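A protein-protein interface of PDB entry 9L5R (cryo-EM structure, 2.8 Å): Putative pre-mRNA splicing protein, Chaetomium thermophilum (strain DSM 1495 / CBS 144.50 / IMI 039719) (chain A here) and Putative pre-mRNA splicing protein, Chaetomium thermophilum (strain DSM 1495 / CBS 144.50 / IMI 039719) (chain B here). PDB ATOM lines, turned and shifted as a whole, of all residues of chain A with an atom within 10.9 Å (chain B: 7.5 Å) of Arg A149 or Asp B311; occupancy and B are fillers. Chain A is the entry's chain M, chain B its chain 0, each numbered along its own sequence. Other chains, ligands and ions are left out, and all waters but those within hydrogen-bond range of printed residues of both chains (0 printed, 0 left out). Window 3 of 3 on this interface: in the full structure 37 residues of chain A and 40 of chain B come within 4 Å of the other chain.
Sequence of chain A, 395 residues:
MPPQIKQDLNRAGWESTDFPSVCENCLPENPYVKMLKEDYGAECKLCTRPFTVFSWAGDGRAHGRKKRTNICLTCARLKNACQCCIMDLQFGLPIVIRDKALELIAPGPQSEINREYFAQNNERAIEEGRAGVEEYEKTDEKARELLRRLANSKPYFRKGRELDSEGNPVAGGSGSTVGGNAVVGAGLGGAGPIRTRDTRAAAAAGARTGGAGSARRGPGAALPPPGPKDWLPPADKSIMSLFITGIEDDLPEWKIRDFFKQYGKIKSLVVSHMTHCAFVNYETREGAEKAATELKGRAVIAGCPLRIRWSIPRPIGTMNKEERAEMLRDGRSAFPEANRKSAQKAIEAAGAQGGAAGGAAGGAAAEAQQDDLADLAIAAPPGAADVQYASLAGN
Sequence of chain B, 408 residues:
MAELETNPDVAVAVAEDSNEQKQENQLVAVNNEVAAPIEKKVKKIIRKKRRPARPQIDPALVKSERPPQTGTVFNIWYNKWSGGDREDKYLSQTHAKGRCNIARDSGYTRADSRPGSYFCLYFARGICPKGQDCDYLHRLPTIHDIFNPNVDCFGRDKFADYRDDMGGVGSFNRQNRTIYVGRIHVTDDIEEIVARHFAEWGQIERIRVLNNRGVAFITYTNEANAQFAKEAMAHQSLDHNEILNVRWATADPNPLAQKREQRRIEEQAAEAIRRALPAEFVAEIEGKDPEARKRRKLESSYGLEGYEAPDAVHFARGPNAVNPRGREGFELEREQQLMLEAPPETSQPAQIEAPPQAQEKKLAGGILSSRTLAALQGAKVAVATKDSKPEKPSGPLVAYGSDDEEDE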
ATOM      1  N   ALA A 101      -6.917 -29.516 -30.922  1.00  0.00           N
ATOM      2  CA  ALA A 101      -7.956 -28.678 -30.342  1.00  0.00           C
ATOM      3  C   ALA A 101      -8.459 -29.224 -29.008  1.00  0.00           C
ATOM      4  O   ALA A 101      -8.726 -28.450 -28.085  1.00  0.00           O
ATOM      5  CB  ALA A 101      -9.095 -28.535 -31.338  1.00  0.00           C
ATOM      6  N   LEU A 102      -8.567 -30.545 -28.876  1.00  0.00           N
ATOM      7  CA  LEU A 102      -8.962 -31.206 -27.640  1.00  0.00           C
ATOM      8  C   LEU A 102      -7.766 -31.974 -27.119  1.00  0.00           C
ATOM      9  O   LEU A 102      -7.889 -33.162 -26.808  1.00  0.00           O
ATOM     10  CB  LEU A 102     -10.117 -32.184 -27.850  1.00  0.00           C
ATOM     11  CG  LEU A 102     -11.383 -31.804 -28.598  1.00  0.00           C
ATOM     12  CD1 LEU A 102     -12.171 -33.040 -28.958  1.00  0.00           C
ATOM     13  CD2 LEU A 102     -12.174 -30.965 -27.676  1.00  0.00           C
ATOM     14  N   ASP A 140     -14.505 -37.719 -23.857  1.00  0.00           N
ATOM     15  CA  ASP A 140     -14.157 -36.390 -24.346  1.00  0.00           C
ATOM     16  C   ASP A 140     -15.352 -35.454 -24.468  1.00  0.00           C
ATOM     17  O   ASP A 140     -15.217 -34.381 -25.077  1.00  0.00           O
ATOM     18  CB  ASP A 140     -13.454 -36.495 -25.701  1.00  0.00           C
ATOM     19  CG  ASP A 140     -14.352 -37.055 -26.775  1.00  0.00           C
ATOM     20  OD1 ASP A 140     -15.181 -37.928 -26.458  1.00  0.00           O
ATOM     21  OD2 ASP A 140     -14.227 -36.629 -27.938  1.00  0.00           O
ATOM     22  N   GLU A 141     -16.508 -35.832 -23.912  1.00  0.00           N
ATOM     23  CA  GLU A 141     -17.648 -34.925 -23.814  1.00  0.00           C
ATOM     24  C   GLU A 141     -17.265 -33.643 -23.096  1.00  0.00           C
ATOM     25  O   GLU A 141     -17.532 -32.538 -23.586  1.00  0.00           O
ATOM     26  CB  GLU A 141     -18.809 -35.602 -23.079  1.00  0.00           C
ATOM     27  CG  GLU A 141     -19.470 -36.773 -23.787  1.00  0.00           C
ATOM     28  CD  GLU A 141     -18.738 -38.084 -23.601  1.00  0.00           C
ATOM     29  OE1 GLU A 141     -17.734 -38.117 -22.861  1.00  0.00           O
ATOM     30  OE2 GLU A 141     -19.167 -39.086 -24.204  1.00  0.00           O
ATOM     31  N   LYS A 142     -16.632 -33.785 -21.929  1.00  0.00           N
ATOM     32  CA  LYS A 142     -16.163 -32.630 -21.175  1.00  0.00           C
ATOM     33  C   LYS A 142     -15.171 -31.816 -21.987  1.00  0.00           C
ATOM     34  O   LYS A 142     -15.195 -30.583 -21.947  1.00  0.00           O
ATOM     35  CB  LYS A 142     -15.531 -33.091 -19.864  1.00  0.00           C
ATOM     36  CG  LYS A 142     -16.476 -33.866 -18.966  1.00  0.00           C
ATOM     37  CD  LYS A 142     -17.241 -32.949 -18.026  1.00  0.00           C
ATOM     38  CE  LYS A 142     -16.451 -32.658 -16.759  1.00  0.00           C
ATOM     39  NZ  LYS A 142     -17.304 -32.055 -15.699  1.00  0.00           N
ATOM     40  N   ALA A 143     -14.328 -32.494 -22.767  1.00  0.00           N
ATOM     41  CA  ALA A 143     -13.318 -31.807 -23.563  1.00  0.00           C
ATOM     42  C   ALA A 143     -13.948 -30.911 -24.620  1.00  0.00           C
ATOM     43  O   ALA A 143     -13.551 -29.750 -24.773  1.00  0.00           O
ATOM     44  CB  ALA A 143     -12.379 -32.824 -24.203  1.00  0.00           C
ATOM     45  N   ARG A 144     -14.949 -31.407 -25.353  1.00  0.00           N
ATOM     46  CA  ARG A 144     -15.481 -30.475 -26.340  1.00  0.00           C
ATOM     47  C   ARG A 144     -16.503 -29.492 -25.787  1.00  0.00           C
ATOM     48  O   ARG A 144     -16.653 -28.404 -26.367  1.00  0.00           O
ATOM     49  CB  ARG A 144     -16.029 -31.150 -27.598  1.00  0.00           C
ATOM     50  CG  ARG A 144     -17.333 -31.922 -27.652  1.00  0.00           C
ATOM     51  CD  ARG A 144     -17.355 -33.340 -27.172  1.00  0.00           C
ATOM     52  NE  ARG A 144     -18.634 -33.906 -27.596  1.00  0.00           N
ATOM     53  CZ  ARG A 144     -19.136 -35.079 -27.239  1.00  0.00           C
ATOM     54  NH1 ARG A 144     -18.371 -36.037 -26.749  1.00  0.00           N
ATOM     55  NH2 ARG A 144     -20.414 -35.340 -27.492  1.00  0.00           N
ATOM     56  N   GLU A 145     -17.156 -29.801 -24.663  1.00  0.00           N
ATOM     57  CA  GLU A 145     -17.919 -28.767 -23.970  1.00  0.00           C
ATOM     58  C   GLU A 145     -17.008 -27.610 -23.559  1.00  0.00           C
ATOM     59  O   GLU A 145     -17.315 -26.438 -23.825  1.00  0.00           O
ATOM     60  CB  GLU A 145     -18.638 -29.364 -22.759  1.00  0.00           C
ATOM     61  CG  GLU A 145     -19.791 -30.302 -23.099  1.00  0.00           C
ATOM     62  CD  GLU A 145     -20.059 -31.324 -22.005  1.00  0.00           C
ATOM     63  OE1 GLU A 145     -19.464 -31.201 -20.918  1.00  0.00           O
ATOM     64  OE2 GLU A 145     -20.862 -32.253 -22.230  1.00  0.00           O
ATOM     65  N   LEU A 146     -15.843 -27.932 -22.979  1.00  0.00           N
ATOM     66  CA  LEU A 146     -14.867 -26.904 -22.626  1.00  0.00           C
ATOM     67  C   LEU A 146     -14.351 -26.161 -23.851  1.00  0.00           C
ATOM     68  O   LEU A 146     -14.110 -24.952 -23.780  1.00  0.00           O
ATOM     69  CB  LEU A 146     -13.692 -27.511 -21.858  1.00  0.00           C
ATOM     70  CG  LEU A 146     -13.877 -28.107 -20.462  1.00  0.00           C
ATOM     71  CD1 LEU A 146     -12.587 -28.763 -19.993  1.00  0.00           C
ATOM     72  CD2 LEU A 146     -14.317 -27.035 -19.475  1.00  0.00           C
ATOM     73  N   LEU A 147     -14.148 -26.863 -24.972  1.00  0.00           N
ATOM     74  CA  LEU A 147     -13.654 -26.186 -26.170  1.00  0.00           C
ATOM     75  C   LEU A 147     -14.642 -25.149 -26.674  1.00  0.00           C
ATOM     76  O   LEU A 147     -14.242 -24.059 -27.095  1.00  0.00           O
ATOM     77  CB  LEU A 147     -13.328 -27.192 -27.277  1.00  0.00           C
ATOM     78  CG  LEU A 147     -12.640 -26.638 -28.539  1.00  0.00           C
ATOM     79  CD1 LEU A 147     -11.799 -27.693 -29.113  1.00  0.00           C
ATOM     80  CD2 LEU A 147     -13.600 -26.229 -29.638  1.00  0.00           C
ATOM     81  N   ARG A 148     -15.928 -25.474 -26.674  1.00  0.00           N
ATOM     82  CA  ARG A 148     -16.892 -24.477 -27.124  1.00  0.00           C
ATOM     83  C   ARG A 148     -17.063 -23.331 -26.137  1.00  0.00           C
ATOM     84  O   ARG A 148     -17.262 -22.183 -26.568  1.00  0.00           O
ATOM     85  CB  ARG A 148     -18.208 -25.162 -27.446  1.00  0.00           C
ATOM     86  CG  ARG A 148     -18.072 -26.018 -28.671  1.00  0.00           C
ATOM     87  CD  ARG A 148     -19.368 -26.646 -29.024  1.00  0.00           C
ATOM     88  NE  ARG A 148     -19.687 -27.644 -28.017  1.00  0.00           N
ATOM     89  CZ  ARG A 148     -20.690 -27.570 -27.159  1.00  0.00           C
ATOM     90  NH1 ARG A 148     -21.506 -26.530 -27.140  1.00  0.00           N
ATOM     91  NH2 ARG A 148     -20.873 -28.564 -26.298  1.00  0.00           N
ATOM     92  N   ARG A 149     -16.930 -23.601 -24.832  1.00  0.00           N
ATOM     93  CA  ARG A 149     -16.854 -22.511 -23.857  1.00  0.00           C
ATOM     94  C   ARG A 149     -15.684 -21.576 -24.161  1.00  0.00           C
ATOM     95  O   ARG A 149     -15.838 -20.347 -24.176  1.00  0.00           O
ATOM     96  CB  ARG A 149     -16.714 -23.077 -22.442  1.00  0.00           C
ATOM     97  CG  ARG A 149     -17.993 -23.139 -21.628  1.00  0.00           C
ATOM     98  CD  ARG A 149     -18.884 -24.240 -22.130  1.00  0.00           C
ATOM     99  NE  ARG A 149     -19.885 -24.666 -21.161  1.00  0.00           N
ATOM    100  CZ  ARG A 149     -19.726 -25.678 -20.318  1.00  0.00           C
ATOM    101  NH1 ARG A 149     -18.587 -26.345 -20.247  1.00  0.00           N
ATOM    102  NH2 ARG A 149     -20.737 -26.031 -19.529  1.00  0.00           N
ATOM    103  N   LEU A 150     -14.506 -22.147 -24.420  1.00  0.00           N
ATOM    104  CA  LEU A 150     -13.320 -21.339 -24.691  1.00  0.00           C
ATOM    105  C   LEU A 150     -13.450 -20.557 -25.994  1.00  0.00           C
ATOM    106  O   LEU A 150     -13.080 -19.380 -26.058  1.00  0.00           O
ATOM    107  CB  LEU A 150     -12.081 -22.230 -24.731  1.00  0.00           C
ATOM    108  CG  LEU A 150     -11.218 -22.290 -23.471  1.00  0.00           C
ATOM    109  CD1 LEU A 150     -11.942 -23.006 -22.349  1.00  0.00           C
ATOM    110  CD2 LEU A 150      -9.894 -22.966 -23.771  1.00  0.00           C
ATOM    111  N   ALA A 151     -13.983 -21.191 -27.040  1.00  0.00           N
ATOM    112  CA  ALA A 151     -14.078 -20.534 -28.340  1.00  0.00           C
ATOM    113  C   ALA A 151     -15.132 -19.438 -28.342  1.00  0.00           C
ATOM    114  O   ALA A 151     -15.045 -18.501 -29.142  1.00  0.00           O
ATOM    115  CB  ALA A 151     -14.373 -21.562 -29.431  1.00  0.00           C
ATOM    116  N   ASN A 152     -16.149 -19.549 -27.488  1.00  0.00           N
ATOM    117  CA  ASN A 152     -17.110 -18.462 -27.348  1.00  0.00           C
ATOM    118  C   ASN A 152     -16.723 -17.438 -26.295  1.00  0.00           C
ATOM    119  O   ASN A 152     -17.383 -16.398 -26.191  1.00  0.00           O
ATOM    120  CB  ASN A 152     -18.470 -19.068 -27.092  1.00  0.00           C
ATOM    121  CG  ASN A 152     -18.984 -19.744 -28.317  1.00  0.00           C
ATOM    122  OD1 ASN A 152     -19.529 -20.841 -28.232  1.00  0.00           O
ATOM    123  ND2 ASN A 152     -19.020 -19.020 -29.403  1.00  0.00           N
ATOM    124  N   SER A 153     -15.694 -17.712 -25.496  1.00  0.00           N
ATOM    125  CA  SER A 153     -14.951 -16.619 -24.883  1.00  0.00           C
ATOM    126  C   SER A 153     -14.183 -15.892 -25.982  1.00  0.00           C
ATOM    127  O   SER A 153     -13.189 -16.409 -26.502  1.00  0.00           O
ATOM    128  CB  SER A 153     -14.004 -17.126 -23.797  1.00  0.00           C
ATOM    129  OG  SER A 153     -13.411 -16.043 -23.104  1.00  0.00           O
ATOM    130  N   LYS A 154     -14.645 -14.701 -26.350  1.00  0.00           N
ATOM    131  CA  LYS A 154     -14.132 -14.001 -27.517  1.00  0.00           C
ATOM    132  C   LYS A 154     -12.760 -13.377 -27.245  1.00  0.00           C
ATOM    133  O   LYS A 154     -12.397 -13.135 -26.091  1.00  0.00           O
ATOM    134  CB  LYS A 154     -15.132 -12.929 -27.944  1.00  0.00           C
ATOM    135  CG  LYS A 154     -16.530 -13.461 -28.175  1.00  0.00           C
ATOM    136  CD  LYS A 154     -17.559 -12.349 -28.081  1.00  0.00           C
ATOM    137  CE  LYS A 154     -18.972 -12.907 -28.036  1.00  0.00           C
ATOM    138  NZ  LYS A 154     -19.983 -11.876 -27.665  1.00  0.00           N
ATOM    139  N   PRO A 155     -11.968 -13.096 -28.304  1.00  0.00           N
ATOM    140  CA  PRO A 155     -10.681 -12.438 -28.043  1.00  0.00           C
ATOM    141  C   PRO A 155     -10.834 -10.982 -27.618  1.00  0.00           C
ATOM    142  O   PRO A 155     -10.654 -10.689 -26.437  1.00  0.00           O
ATOM    143  CB  PRO A 155      -9.962 -12.526 -29.391  1.00  0.00           C
ATOM    144  CG  PRO A 155     -11.055 -12.574 -30.386  1.00  0.00           C
ATOM    145  CD  PRO A 155     -12.128 -13.406 -29.739  1.00  0.00           C
ATOM    146  N   GLU B 284     -27.380 -24.226 -25.029  1.00  0.00           N
ATOM    147  CA  GLU B 284     -27.312 -24.382 -23.580  1.00  0.00           C
ATOM    148  C   GLU B 284     -25.872 -24.411 -23.082  1.00  0.00           C
ATOM    149  O   GLU B 284     -25.564 -23.838 -22.032  1.00  0.00           O
ATOM    150  CB  GLU B 284     -28.051 -25.651 -23.159  1.00  0.00           C
ATOM    151  CG  GLU B 284     -29.565 -25.512 -23.143  1.00  0.00           C
ATOM    152  CD  GLU B 284     -30.260 -26.721 -22.549  1.00  0.00           C
ATOM    153  OE1 GLU B 284     -29.622 -27.787 -22.445  1.00  0.00           O
ATOM    154  OE2 GLU B 284     -31.448 -26.609 -22.185  1.00  0.00           O
ATOM    155  N   ILE B 285     -24.975 -25.071 -23.815  1.00  0.00           N
ATOM    156  CA  ILE B 285     -23.591 -25.158 -23.370  1.00  0.00           C
ATOM    157  C   ILE B 285     -22.856 -23.852 -23.645  1.00  0.00           C
ATOM    158  O   ILE B 285     -22.027 -23.411 -22.839  1.00  0.00           O
ATOM    159  CB  ILE B 285     -22.913 -26.373 -24.026  1.00  0.00           C
ATOM    160  CG1 ILE B 285     -23.464 -27.629 -23.369  1.00  0.00           C
ATOM    161  CG2 ILE B 285     -21.418 -26.352 -23.816  1.00  0.00           C
ATOM    162  CD1 ILE B 285     -23.213 -28.912 -24.089  1.00  0.00           C
ATOM    163  N   GLU B 286     -23.169 -23.196 -24.765  1.00  0.00           N
ATOM    164  CA  GLU B 286     -22.504 -21.944 -25.105  1.00  0.00           C
ATOM    165  C   GLU B 286     -22.855 -20.856 -24.100  1.00  0.00           C
ATOM    166  O   GLU B 286     -21.965 -20.196 -23.552  1.00  0.00           O
ATOM    167  CB  GLU B 286     -22.895 -21.509 -26.517  1.00  0.00           C
ATOM    168  CG  GLU B 286     -22.144 -22.231 -27.603  1.00  0.00           C
ATOM    169  CD  GLU B 286     -22.486 -21.743 -28.996  1.00  0.00           C
ATOM    170  OE1 GLU B 286     -23.522 -21.070 -29.167  1.00  0.00           O
ATOM    171  OE2 GLU B 286     -21.700 -22.024 -29.924  1.00  0.00           O
ATOM    172  N   GLY B 287     -24.148 -20.677 -23.827  1.00  0.00           N
ATOM    173  CA  GLY B 287     -24.567 -19.759 -22.786  1.00  0.00           C
ATOM    174  C   GLY B 287     -24.249 -18.305 -23.036  1.00  0.00           C
ATOM    175  O   GLY B 287     -24.044 -17.554 -22.081  1.00  0.00           O
ATOM    176  N   ARG B 296     -31.282 -23.564 -19.601  1.00  0.00           N
ATOM    177  CA  ARG B 296     -30.286 -24.447 -19.005  1.00  0.00           C
ATOM    178  C   ARG B 296     -30.552 -24.653 -17.518  1.00  0.00           C
ATOM    179  O   ARG B 296     -30.537 -25.794 -17.040  1.00  0.00           O
ATOM    180  CB  ARG B 296     -28.877 -23.900 -19.241  1.00  0.00           C
ATOM    181  CG  ARG B 296     -27.805 -24.518 -18.359  1.00  0.00           C
ATOM    182  CD  ARG B 296     -27.344 -25.849 -18.917  1.00  0.00           C
ATOM    183  NE  ARG B 296     -26.000 -26.203 -18.479  1.00  0.00           N
ATOM    184  CZ  ARG B 296     -25.725 -27.156 -17.599  1.00  0.00           C
ATOM    185  NH1 ARG B 296     -26.683 -27.866 -17.028  1.00  0.00           N
ATOM    186  NH2 ARG B 296     -24.457 -27.403 -17.286  1.00  0.00           N
ATOM    187  N   SER B 300     -31.862 -28.279 -16.277  1.00  0.00           N
ATOM    188  CA  SER B 300     -30.955 -28.935 -15.349  1.00  0.00           C
ATOM    189  C   SER B 300     -31.557 -29.067 -13.961  1.00  0.00           C
ATOM    190  O   SER B 300     -31.106 -29.912 -13.182  1.00  0.00           O
ATOM    191  CB  SER B 300     -29.640 -28.166 -15.283  1.00  0.00           C
ATOM    192  OG  SER B 300     -28.840 -28.631 -14.216  1.00  0.00           O
ATOM    193  N   GLU B 308     -29.004 -28.164 -10.182  1.00  0.00           N
ATOM    194  CA  GLU B 308     -27.891 -27.991 -11.128  1.00  0.00           C
ATOM    195  C   GLU B 308     -27.228 -29.334 -11.485  1.00  0.00           C
ATOM    196  O   GLU B 308     -26.115 -29.658 -11.074  1.00  0.00           O
ATOM    197  CB  GLU B 308     -26.882 -26.901 -10.687  1.00  0.00           C
ATOM    198  CG  GLU B 308     -25.948 -27.051  -9.445  1.00  0.00           C
ATOM    199  CD  GLU B 308     -26.549 -26.625  -8.108  1.00  0.00           C
ATOM    200  OE1 GLU B 308     -27.774 -26.459  -7.988  1.00  0.00           O
ATOM    201  OE2 GLU B 308     -25.766 -26.462  -7.149  1.00  0.00           O
ATOM    202  N   ALA B 309     -28.002 -30.141 -12.234  1.00  0.00           N
ATOM    203  CA  ALA B 309     -27.633 -31.456 -12.764  1.00  0.00           C
ATOM    204  C   ALA B 309     -26.231 -31.502 -13.357  1.00  0.00           C
ATOM    205  O   ALA B 309     -25.758 -30.500 -13.908  1.00  0.00           O
ATOM    206  CB  ALA B 309     -28.627 -31.899 -13.837  1.00  0.00           C
ATOM    207  N   PRO B 310     -25.535 -32.635 -13.242  1.00  0.00           N
ATOM    208  CA  PRO B 310     -24.211 -32.756 -13.861  1.00  0.00           C
ATOM    209  C   PRO B 310     -24.292 -32.627 -15.371  1.00  0.00           C
ATOM    210  O   PRO B 310     -25.309 -32.942 -15.989  1.00  0.00           O
ATOM    211  CB  PRO B 310     -23.756 -34.160 -13.449  1.00  0.00           C
ATOM    212  CG  PRO B 310     -24.530 -34.459 -12.220  1.00  0.00           C
ATOM    213  CD  PRO B 310     -25.855 -33.799 -12.401  1.00  0.00           C
ATOM    214  N   ASP B 311     -23.205 -32.122 -15.958  1.00  0.00           N
ATOM    215  CA  ASP B 311     -23.147 -31.978 -17.407  1.00  0.00           C
ATOM    216  C   ASP B 311     -23.236 -33.332 -18.093  1.00  0.00           C
ATOM    217  O   ASP B 311     -23.867 -33.457 -19.146  1.00  0.00           O
ATOM    218  CB  ASP B 311     -21.868 -31.252 -17.816  1.00  0.00           C
ATOM    219  CG  ASP B 311     -21.935 -29.764 -17.552  1.00  0.00           C
ATOM    220  OD1 ASP B 311     -22.840 -29.336 -16.807  1.00  0.00           O
ATOM    221  OD2 ASP B 311     -21.085 -29.024 -18.087  1.00  0.00           O
ATOM    222  N   ALA B 312     -22.629 -34.360 -17.495  1.00  0.00           N
ATOM    223  CA  ALA B 312     -22.700 -35.706 -18.055  1.00  0.00           C
ATOM    224  C   ALA B 312     -24.131 -36.226 -18.093  1.00  0.00           C
ATOM    225  O   ALA B 312     -24.564 -36.783 -19.105  1.00  0.00           O
ATOM    226  CB  ALA B 312     -21.812 -36.653 -17.248  1.00  0.00           C
ATOM    227  N   VAL B 313     -24.885 -36.033 -17.010  1.00  0.00           N
ATOM    228  CA  VAL B 313     -26.268 -36.497 -16.977  1.00  0.00           C
ATOM    229  C   VAL B 313     -27.131 -35.668 -17.916  1.00  0.00           C
ATOM    230  O   VAL B 313     -28.005 -36.199 -18.611  1.00  0.00           O
ATOM    231  CB  VAL B 313     -26.820 -36.459 -15.541  1.00  0.00           C
ATOM    232  CG1 VAL B 313     -28.186 -37.114 -15.486  1.00  0.00           C
ATOM    233  CG2 VAL B 313     -25.868 -37.115 -14.577  1.00  0.00           C
ATOM    234  N   HIS B 314     -26.901 -34.358 -17.959  1.00  0.00           N
ATOM    235  CA  HIS B 314     -27.780 -33.487 -18.724  1.00  0.00           C
ATOM    236  C   HIS B 314     -27.526 -33.566 -20.221  1.00  0.00           C
ATOM    237  O   HIS B 314     -28.454 -33.357 -21.009  1.00  0.00           O
ATOM    238  CB  HIS B 314     -27.639 -32.046 -18.253  1.00  0.00           C
ATOM    239  CG  HIS B 314     -28.738 -31.157 -18.731  1.00  0.00           C
ATOM    240  ND1 HIS B 314     -30.062 -31.538 -18.702  1.00  0.00           N
ATOM    241  CD2 HIS B 314     -28.715 -29.913 -19.259  1.00  0.00           C
ATOM    242  CE1 HIS B 314     -30.807 -30.564 -19.192  1.00  0.00           C
ATOM    243  NE2 HIS B 314     -30.014 -29.567 -19.538  1.00  0.00           N
ATOM    244  N   PHE B 315     -26.297 -33.851 -20.638  1.00  0.00           N
ATOM    245  CA  PHE B 315     -25.959 -33.930 -22.049  1.00  0.00           C
ATOM    246  C   PHE B 315     -25.600 -35.342 -22.484  1.00  0.00           C
ATOM    247  O   PHE B 315     -25.040 -35.520 -23.570  1.00  0.00           O
ATOM    248  CB  PHE B 315     -24.817 -32.964 -22.357  1.00  0.00           C
ATOM    249  CG  PHE B 315     -25.086 -31.567 -21.899  1.00  0.00           C
ATOM    250  CD1 PHE B 315     -26.257 -30.926 -22.253  1.00  0.00           C
ATOM    251  CD2 PHE B 315     -24.191 -30.911 -21.076  1.00  0.00           C
ATOM    252  CE1 PHE B 315     -26.516 -29.646 -21.823  1.00  0.00           C
ATOM    253  CE2 PHE B 315     -24.448 -29.636 -20.635  1.00  0.00           C
ATOM    254  CZ  PHE B 315     -25.616 -29.004 -21.007  1.00  0.00           C
ATOM    255  N   ALA B 316     -25.897 -36.346 -21.664  1.00  0.00           N
ATOM    256  CA  ALA B 316     -25.700 -37.736 -22.056  1.00  0.00           C
ATOM    257  C   ALA B 316     -26.718 -38.075 -23.129  1.00  0.00           C
ATOM    258  O   ALA B 316     -27.898 -38.276 -22.842  1.00  0.00           O
ATOM    259  CB  ALA B 316     -25.837 -38.658 -20.854  1.00  0.00           C
ATOM    260  N   ARG B 317     -26.264 -38.133 -24.374  1.00  0.00           N
ATOM    261  CA  ARG B 317     -27.164 -38.382 -25.484  1.00  0.00           C
ATOM    262  C   ARG B 317     -27.448 -39.866 -25.631  1.00  0.00           C
ATOM    263  O   ARG B 317     -26.614 -40.721 -25.320  1.00  0.00           O
ATOM    264  CB  ARG B 317     -26.589 -37.829 -26.784  1.00  0.00           C
ATOM    265  CG  ARG B 317     -26.530 -36.324 -26.805  1.00  0.00           C
ATOM    266  CD  ARG B 317     -25.534 -35.785 -27.826  1.00  0.00           C
ATOM    267  NE  ARG B 317     -25.612 -36.437 -29.129  1.00  0.00           N
ATOM    268  CZ  ARG B 317     -26.612 -36.313 -29.993  1.00  0.00           C
ATOM    269  NH1 ARG B 317     -27.698 -35.617 -29.708  1.00  0.00           N
ATOM    270  NH2 ARG B 317     -26.524 -36.912 -31.174  1.00  0.00           N
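Of the 16 printed residues of chain B, 4 touch a printed residue of chain A.
Printed residues of chain B that touch a printed residue of chain A: Ile B285, Glu B286, Asp B311 and Phe B315.
Of the 18 printed residues of chain A, 4 touch a printed residue of chain B.
Printed residues of chain A that touch a printed residue of chain B: Glu A145, Arg A148, Arg A149 and Asn A152.
Along chain A the printed residues that touch a printed residue of chain B span positions 145 to 152.
Among the printed residues, 7 pairs touch across the chains.
Among the printed residues, Asp or Glu carboxylates within 4 Å of a Lys or Arg side-chain nitrogen of the other chain: Arg A149 with Asp B311 (3.3 Å).
Arg A144 touches none of the printed residues of chain B.
Of the printed residues of chain B, Arg A148 touches Ile B285 (3.2 Å).
Arg A149 touches just these residues of chain B: Ile B285 (3.0 Å) and Asp B311 (3.3 Å).
Printed residues of chain A within 4 Å of Glu B286: Asn A152 (3.0 Å).
No residue of chain A comes within 4 Å of Ala B309.
Asp B311 touches two residues of chain A.
No residue of chain A comes within 4 Å of Ala B312.
No residue of chain A comes within 4 Å of Val B313.
Phe B315 touches one residue of chain A.
The nearest printed residue of chain B that does not touch Asn A152 is Gly B287 (6.4 Å).
O of Arg A148 sits close to OD1 of Asn A152 (3.1 Å).
The side-chain carboxylate (OD1) of Asp B311 lies within salt-bridge range of the guanidinium group (NH2) of Arg B296, at 2.6 Å.
OE2 of Glu B286 sits close to OD1 of Asn A152.
NE of Arg A149 is in hydrogen-bond range of O of Ile B285 (3.0 Å).
The side-chain carboxylate of Asp B311 is in salt-bridge range of the guanidinium group of Arg A149.
Ile B285 touches Glu A145 (CD1 to CG, 3.8 Å).
OD2 of Asp B311 touches OE1 of Glu A145, at 3.9 Å.
OE2 of Glu A145 touches CD2 of Phe B315, at 3.8 Å.
CD1 of Ile B285 touches NH2 of Arg A148, 3.2 Å away.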
